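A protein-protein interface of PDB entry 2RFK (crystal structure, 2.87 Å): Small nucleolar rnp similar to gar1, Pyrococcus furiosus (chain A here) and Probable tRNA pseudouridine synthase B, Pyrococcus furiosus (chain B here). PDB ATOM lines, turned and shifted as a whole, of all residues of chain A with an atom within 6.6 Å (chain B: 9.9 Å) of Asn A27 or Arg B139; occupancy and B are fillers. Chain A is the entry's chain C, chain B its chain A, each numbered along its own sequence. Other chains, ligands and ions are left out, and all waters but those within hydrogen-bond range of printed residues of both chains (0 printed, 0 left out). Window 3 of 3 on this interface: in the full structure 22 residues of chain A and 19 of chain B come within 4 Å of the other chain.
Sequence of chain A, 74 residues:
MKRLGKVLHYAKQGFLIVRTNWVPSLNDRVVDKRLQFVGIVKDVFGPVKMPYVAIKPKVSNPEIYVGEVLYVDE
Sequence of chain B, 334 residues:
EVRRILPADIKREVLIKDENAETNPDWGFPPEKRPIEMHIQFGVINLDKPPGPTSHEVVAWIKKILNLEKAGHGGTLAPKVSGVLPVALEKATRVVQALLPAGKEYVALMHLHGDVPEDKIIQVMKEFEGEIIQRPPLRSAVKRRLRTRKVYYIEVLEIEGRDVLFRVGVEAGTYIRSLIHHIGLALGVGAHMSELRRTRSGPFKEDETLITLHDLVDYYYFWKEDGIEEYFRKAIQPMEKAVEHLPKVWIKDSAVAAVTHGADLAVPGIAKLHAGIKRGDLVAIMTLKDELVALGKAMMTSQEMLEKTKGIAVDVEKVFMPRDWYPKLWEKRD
NH2 of Arg B139 lies close to ND2 of Asn A27.
O of Leu B138 sits close to O of Leu A26, at 3.4 Å.
OG of Ser A25 lies within hydrogen-bond range of OD1 of Asp A28.
O of Asn A27 is in hydrogen-bond range of NH2 of Arg A29, at 2.7 Å.
Among the printed residues, merely in contact across the chains: Ser A25 with Leu B138, Leu A26 with Arg B139, Ser A25 with Pro B137, Leu A26 with Pro B136, Lys A42 with Pro B136 and Leu A26 with Pro B137.
Asn A27 touches just one residue of chain B: Arg B139.
Arg B139 touches two residues of chain A.
No residue of chain B comes within 4 Å of Asp A28.
No residue of chain B comes within 4 Å of Val A41.
Of the printed residues of chain A, Pro B137 touches Ser A25 (3.5 Å) and Leu A26 (3.9 Å).
Of the printed residues of chain A, Leu B138 touches Ser A25 (3.1 Å) and Leu A26 (3.4 Å).
Printed residues of chain B within 4 Å of Ser A25: Pro B137 and Leu B138.
Of the printed residues of chain B, Lys A42 touches Pro B136 (3.9 Å).
The nearest residue of chain B that does not touch Asn A27 is Leu B138 (5.7 Å).
Of the 11 printed residues of chain B, 4 touch a printed residue of chain A.
Printed residues of chain B that touch a printed residue of chain A: Pro B136, Pro B137, Leu B138 and Arg B139.
Hydrophobic or aromatic side chains of chain B that line the printed part of chain A: Pro B136, Pro B137 and Leu B138.
Of the 11 printed residues of chain A, 4 touch a printed residue of chain B.
Printed residues of chain A that touch a printed residue of chain B: Ser A25, Leu A26, Asn A27 and Lys A42.
Hydrophobic or aromatic side chains of chain A that line the printed part of chain B: Leu A26.
Along chain A the printed residues that touch a printed residue of chain B span positions 25 to 42.
Among the printed residues, no Asp or Glu carboxylate lies within 4 Å of a Lys or Arg side-chain nitrogen of the other chain.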
ATOM      1  N   SER A  25      -8.003  13.820  11.889  1.00  0.00           N
ATOM      2  CA  SER A  25      -8.791  13.588  10.673  1.00  0.00           C
ATOM      3  C   SER A  25     -10.306  13.604  10.915  1.00  0.00           C
ATOM      4  O   SER A  25     -10.760  13.593  12.059  1.00  0.00           O
ATOM      5  CB  SER A  25      -8.398  12.259  10.046  1.00  0.00           C
ATOM      6  OG  SER A  25      -8.380  11.232  11.023  1.00  0.00           O
ATOM      7  N   LEU A  26     -11.075  13.617   9.825  1.00  0.00           N
ATOM      8  CA  LEU A  26     -12.540  13.698   9.884  1.00  0.00           C
ATOM      9  C   LEU A  26     -13.163  12.424  10.462  1.00  0.00           C
ATOM     10  O   LEU A  26     -12.870  11.319   9.995  1.00  0.00           O
ATOM     11  CB  LEU A  26     -13.110  13.966   8.480  1.00  0.00           C
ATOM     12  CG  LEU A  26     -14.372  14.811   8.215  1.00  0.00           C
ATOM     13  CD1 LEU A  26     -15.587  14.450   9.098  1.00  0.00           C
ATOM     14  CD2 LEU A  26     -14.052  16.303   8.303  1.00  0.00           C
ATOM     15  N   ASN A  27     -14.014  12.603  11.475  1.00  0.00           N
ATOM     16  CA  ASN A  27     -14.779  11.525  12.141  1.00  0.00           C
ATOM     17  C   ASN A  27     -14.021  10.676  13.183  1.00  0.00           C
ATOM     18  O   ASN A  27     -14.454   9.561  13.513  1.00  0.00           O
ATOM     19  CB  ASN A  27     -15.519  10.629  11.124  1.00  0.00           C
ATOM     20  CG  ASN A  27     -16.592  11.379  10.348  1.00  0.00           C
ATOM     21  OD1 ASN A  27     -17.346  12.176  10.912  1.00  0.00           O
ATOM     22  ND2 ASN A  27     -16.666  11.123   9.047  1.00  0.00           N
ATOM     23  N   ASP A  28     -12.912  11.208  13.706  1.00  0.00           N
ATOM     24  CA  ASP A  28     -12.156  10.552  14.793  1.00  0.00           C
ATOM     25  C   ASP A  28     -12.863  10.733  16.150  1.00  0.00           C
ATOM     26  O   ASP A  28     -13.286  11.842  16.483  1.00  0.00           O
ATOM     27  CB  ASP A  28     -10.713  11.094  14.867  1.00  0.00           C
ATOM     28  CG  ASP A  28      -9.739  10.371  13.924  1.00  0.00           C
ATOM     29  OD1 ASP A  28      -8.668  10.954  13.628  1.00  0.00           O
ATOM     30  OD2 ASP A  28     -10.024   9.228  13.489  1.00  0.00           O
ATOM     31  N   ARG A  29     -12.984   9.656  16.929  1.00  0.00           N
ATOM     32  CA  ARG A  29     -13.651   9.744  18.231  1.00  0.00           C
ATOM     33  C   ARG A  29     -12.774  10.493  19.228  1.00  0.00           C
ATOM     34  O   ARG A  29     -11.622  10.125  19.457  1.00  0.00           O
ATOM     35  CB  ARG A  29     -14.001   8.362  18.805  1.00  0.00           C
ATOM     36  CG  ARG A  29     -14.302   7.224  17.818  1.00  0.00           C
ATOM     37  CD  ARG A  29     -15.461   7.517  16.879  1.00  0.00           C
ATOM     38  NE  ARG A  29     -15.000   7.658  15.497  1.00  0.00           N
ATOM     39  CZ  ARG A  29     -14.997   6.671  14.604  1.00  0.00           C
ATOM     40  NH1 ARG A  29     -15.441   5.461  14.937  1.00  0.00           N
ATOM     41  NH2 ARG A  29     -14.554   6.894  13.372  1.00  0.00           N
ATOM     42  N   GLY A  39     -16.861  14.051  21.362  1.00  0.00           N
ATOM     43  CA  GLY A  39     -17.471  14.252  20.042  1.00  0.00           C
ATOM     44  C   GLY A  39     -16.752  13.628  18.853  1.00  0.00           C
ATOM     45  O   GLY A  39     -15.909  12.734  19.008  1.00  0.00           O
ATOM     46  N   ILE A  40     -17.126  14.100  17.660  1.00  0.00           N
ATOM     47  CA  ILE A  40     -16.411  13.821  16.407  1.00  0.00           C
ATOM     48  C   ILE A  40     -15.849  15.124  15.825  1.00  0.00           C
ATOM     49  O   ILE A  40     -16.272  16.219  16.216  1.00  0.00           O
ATOM     50  CB  ILE A  40     -17.300  13.083  15.355  1.00  0.00           C
ATOM     51  CG1 ILE A  40     -18.411  13.999  14.815  1.00  0.00           C
ATOM     52  CG2 ILE A  40     -17.847  11.762  15.933  1.00  0.00           C
ATOM     53  CD1 ILE A  40     -19.077  13.487  13.551  1.00  0.00           C
ATOM     54  N   VAL A  41     -14.902  15.000  14.892  1.00  0.00           N
ATOM     55  CA  VAL A  41     -14.224  16.150  14.275  1.00  0.00           C
ATOM     56  C   VAL A  41     -14.940  16.610  12.997  1.00  0.00           C
ATOM     57  O   VAL A  41     -15.717  15.853  12.406  1.00  0.00           O
ATOM     58  CB  VAL A  41     -12.735  15.812  13.953  1.00  0.00           C
ATOM     59  CG1 VAL A  41     -11.966  17.051  13.452  1.00  0.00           C
ATOM     60  CG2 VAL A  41     -12.046  15.220  15.174  1.00  0.00           C
ATOM     61  N   LYS A  42     -14.683  17.854  12.585  1.00  0.00           N
ATOM     62  CA  LYS A  42     -15.176  18.357  11.313  1.00  0.00           C
ATOM     63  C   LYS A  42     -14.117  19.143  10.561  1.00  0.00           C
ATOM     64  O   LYS A  42     -14.268  19.399   9.360  1.00  0.00           O
ATOM     65  CB  LYS A  42     -16.432  19.213  11.503  1.00  0.00           C
ATOM     66  CG  LYS A  42     -17.687  18.430  11.865  1.00  0.00           C
ATOM     67  CD  LYS A  42     -18.179  17.557  10.711  1.00  0.00           C
ATOM     68  CE  LYS A  42     -18.738  16.234  11.214  1.00  0.00           C
ATOM     69  NZ  LYS A  42     -19.677  16.422  12.352  1.00  0.00           N
ATOM     70  N   LYS A  58     -21.541  16.206  20.668  1.00  0.00           N
ATOM     71  CA  LYS A  58     -22.831  15.518  20.536  1.00  0.00           C
ATOM     72  C   LYS A  58     -23.535  15.172  21.866  1.00  0.00           C
ATOM     73  O   LYS A  58     -24.616  14.570  21.873  1.00  0.00           O
ATOM     74  CB  LYS A  58     -22.717  14.307  19.599  1.00  0.00           C
ATOM     75  CG  LYS A  58     -22.853  14.691  18.122  1.00  0.00           C
ATOM     76  CD  LYS A  58     -22.736  13.506  17.186  1.00  0.00           C
ATOM     77  CE  LYS A  58     -21.289  13.130  16.935  1.00  0.00           C
ATOM     78  NZ  LYS A  58     -21.184  12.215  15.775  1.00  0.00           N
ATOM     79  N   GLU A  74      -8.834   6.448  19.055  1.00  0.00           N
ATOM     80  CA  GLU A  74      -8.507   5.953  17.719  1.00  0.00           C
ATOM     81  C   GLU A  74      -9.770   5.747  16.878  1.00  0.00           C
ATOM     82  O   GLU A  74     -10.575   4.840  17.148  1.00  0.00           O
ATOM     83  CB  GLU A  74      -7.682   4.662  17.822  1.00  0.00           C
ATOM     84  CG  GLU A  74      -8.257   3.630  18.775  1.00  0.00           C
ATOM     85  CD  GLU A  74      -7.217   3.079  19.725  1.00  0.00           C
ATOM     86  OE1 GLU A  74      -6.060   2.437  19.040  1.00  0.00           O
ATOM     87  OE2 GLU A  74      -7.613   3.209  21.148  1.00  0.00           O
ATOM     88  OXT GLU A  74     -10.011   6.506  15.926  1.00  0.00           O
ATOM     89  N   ARG B 135      -7.869  20.771   3.973  1.00  0.00           N
ATOM     90  CA  ARG B 135      -8.900  19.719   3.978  1.00  0.00           C
ATOM     91  C   ARG B 135      -8.474  18.660   5.005  1.00  0.00           C
ATOM     92  O   ARG B 135      -7.303  18.279   5.019  1.00  0.00           O
ATOM     93  CB  ARG B 135      -9.039  19.048   2.593  1.00  0.00           C
ATOM     94  CG  ARG B 135      -9.917  17.761   2.598  1.00  0.00           C
ATOM     95  CD  ARG B 135      -9.517  16.694   1.553  1.00  0.00           C
ATOM     96  NE  ARG B 135      -8.130  16.223   1.683  1.00  0.00           N
ATOM     97  CZ  ARG B 135      -7.516  15.395   0.827  1.00  0.00           C
ATOM     98  NH1 ARG B 135      -8.157  14.925  -0.242  1.00  0.00           N
ATOM     99  NH2 ARG B 135      -6.250  15.044   1.028  1.00  0.00           N
ATOM    100  N   PRO B 136      -9.409  18.189   5.870  1.00  0.00           N
ATOM    101  CA  PRO B 136      -9.130  17.053   6.776  1.00  0.00           C
ATOM    102  C   PRO B 136      -8.917  15.688   6.051  1.00  0.00           C
ATOM    103  O   PRO B 136      -9.506  15.474   4.982  1.00  0.00           O
ATOM    104  CB  PRO B 136     -10.374  17.024   7.683  1.00  0.00           C
ATOM    105  CG  PRO B 136     -11.015  18.391   7.516  1.00  0.00           C
ATOM    106  CD  PRO B 136     -10.765  18.728   6.090  1.00  0.00           C
ATOM    107  N   PRO B 137      -8.057  14.786   6.611  1.00  0.00           N
ATOM    108  CA  PRO B 137      -7.710  13.466   6.029  1.00  0.00           C
ATOM    109  C   PRO B 137      -8.507  12.222   6.508  1.00  0.00           C
ATOM    110  O   PRO B 137      -9.734  12.217   6.400  1.00  0.00           O
ATOM    111  CB  PRO B 137      -6.217  13.332   6.380  1.00  0.00           C
ATOM    112  CG  PRO B 137      -6.023  14.199   7.618  1.00  0.00           C
ATOM    113  CD  PRO B 137      -7.276  15.029   7.839  1.00  0.00           C
ATOM    114  N   LEU B 138      -7.793  11.208   7.035  1.00  0.00           N
ATOM    115  CA  LEU B 138      -8.257   9.785   7.320  1.00  0.00           C
ATOM    116  C   LEU B 138      -9.745   9.369   7.088  1.00  0.00           C
ATOM    117  O   LEU B 138     -10.745   9.732   7.829  1.00  0.00           O
ATOM    118  CB  LEU B 138      -7.746   9.266   8.696  1.00  0.00           C
ATOM    119  CG  LEU B 138      -7.741   7.740   9.120  1.00  0.00           C
ATOM    120  CD1 LEU B 138      -6.630   7.424  10.098  1.00  0.00           C
ATOM    121  CD2 LEU B 138      -9.164   7.318   9.645  1.00  0.00           C
ATOM    122  N   ARG B 139      -9.856   8.778   5.763  1.00  0.00           N
ATOM    123  CA  ARG B 139     -11.154   8.503   5.164  1.00  0.00           C
ATOM    124  C   ARG B 139     -11.295   6.983   5.092  1.00  0.00           C
ATOM    125  O   ARG B 139     -11.183   6.274   6.109  1.00  0.00           O
ATOM    126  CB  ARG B 139     -11.198   9.141   3.747  1.00  0.00           C
ATOM    127  CG  ARG B 139     -12.052  10.438   3.570  1.00  0.00           C
ATOM    128  CD  ARG B 139     -11.878  11.478   4.694  1.00  0.00           C
ATOM    129  NE  ARG B 139     -13.159  11.931   5.264  1.00  0.00           N
ATOM    130  CZ  ARG B 139     -13.887  11.257   6.173  1.00  0.00           C
ATOM    131  NH1 ARG B 139     -13.495  10.069   6.647  1.00  0.00           N
ATOM    132  NH2 ARG B 139     -15.030  11.771   6.612  1.00  0.00           N
ATOM    133  N   SER B 140     -11.566   6.497   3.884  1.00  0.00           N
ATOM    134  CA  SER B 140     -11.306   5.116   3.519  1.00  0.00           C
ATOM    135  C   SER B 140      -9.921   5.168   2.885  1.00  0.00           C
ATOM    136  O   SER B 140      -9.117   4.234   3.030  1.00  0.00           O
ATOM    137  CB  SER B 140     -12.339   4.631   2.499  1.00  0.00           C
ATOM    138  OG  SER B 140     -12.390   5.513   1.375  1.00  0.00           O
ATOM    139  N   ALA B 141      -9.669   6.291   2.200  1.00  0.00           N
ATOM    140  CA  ALA B 141      -8.433   6.562   1.469  1.00  0.00           C
ATOM    141  C   ALA B 141      -7.226   6.646   2.399  1.00  0.00           C
ATOM    142  O   ALA B 141      -6.890   7.726   2.897  1.00  0.00           O
ATOM    143  CB  ALA B 141      -8.576   7.865   0.639  1.00  0.00           C
ATOM    144  N   VAL B 142      -6.592   5.497   2.635  1.00  0.00           N
ATOM    145  CA  VAL B 142      -5.332   5.425   3.377  1.00  0.00           C
ATOM    146  C   VAL B 142      -4.259   6.018   2.448  1.00  0.00           C
ATOM    147  O   VAL B 142      -3.702   5.334   1.587  1.00  0.00           O
ATOM    148  CB  VAL B 142      -4.998   3.960   3.860  1.00  0.00           C
ATOM    149  CG1 VAL B 142      -3.867   3.960   4.880  1.00  0.00           C
ATOM    150  CG2 VAL B 142      -6.231   3.276   4.460  1.00  0.00           C
ATOM    151  N   LYS B 143      -4.009   7.311   2.619  1.00  0.00           N
ATOM    152  CA  LYS B 143      -3.257   8.105   1.649  1.00  0.00           C
ATOM    153  C   LYS B 143      -1.735   8.025   1.840  1.00  0.00           C
ATOM    154  O   LYS B 143      -1.243   7.549   2.870  1.00  0.00           O
ATOM    155  CB  LYS B 143      -3.692   9.583   1.725  1.00  0.00           C
ATOM    156  CG  LYS B 143      -5.206   9.895   1.534  1.00  0.00           C
ATOM    157  CD  LYS B 143      -5.290  11.463   0.980  1.00  0.00           C
ATOM    158  CE  LYS B 143      -6.552  12.163   1.648  1.00  0.00           C
ATOM    159  NZ  LYS B 143      -7.821  12.076   0.823  1.00  0.00           N
ATOM    160  N   LEU B 146      -0.648  14.799   1.181  1.00  0.00           N
ATOM    161  CA  LEU B 146      -1.710  15.529   1.893  1.00  0.00           C
ATOM    162  C   LEU B 146      -2.032  16.856   1.240  1.00  0.00           C
ATOM    163  O   LEU B 146      -1.256  17.370   0.417  1.00  0.00           O
ATOM    164  CB  LEU B 146      -1.343  15.773   3.361  1.00  0.00           C
ATOM    165  CG  LEU B 146      -2.487  16.157   4.311  1.00  0.00           C
ATOM    166  CD1 LEU B 146      -2.439  15.299   5.568  1.00  0.00           C
ATOM    167  CD2 LEU B 146      -2.475  17.645   4.650  1.00  0.00           C
ATOM    168  N   ARG B 147      -3.172  17.417   1.636  1.00  0.00           N
ATOM    169  CA  ARG B 147      -3.630  18.707   1.111  1.00  0.00           C
ATOM    170  C   ARG B 147      -3.135  19.958   1.877  1.00  0.00           C
ATOM    171  O   ARG B 147      -3.891  20.638   2.581  1.00  0.00           O
ATOM    172  CB  ARG B 147      -5.148  18.683   0.889  1.00  0.00           C
ATOM    173  CG  ARG B 147      -5.489  18.346  -0.556  1.00  0.00           C
ATOM    174  CD  ARG B 147      -6.946  17.970  -0.797  1.00  0.00           C
ATOM    175  NE  ARG B 147      -7.149  17.585  -2.198  1.00  0.00           N
ATOM    176  CZ  ARG B 147      -6.751  16.430  -2.749  1.00  0.00           C
ATOM    177  NH1 ARG B 147      -6.120  15.486  -2.031  1.00  0.00           N
ATOM    178  NH2 ARG B 147      -6.989  16.220  -4.041  1.00  0.00           N
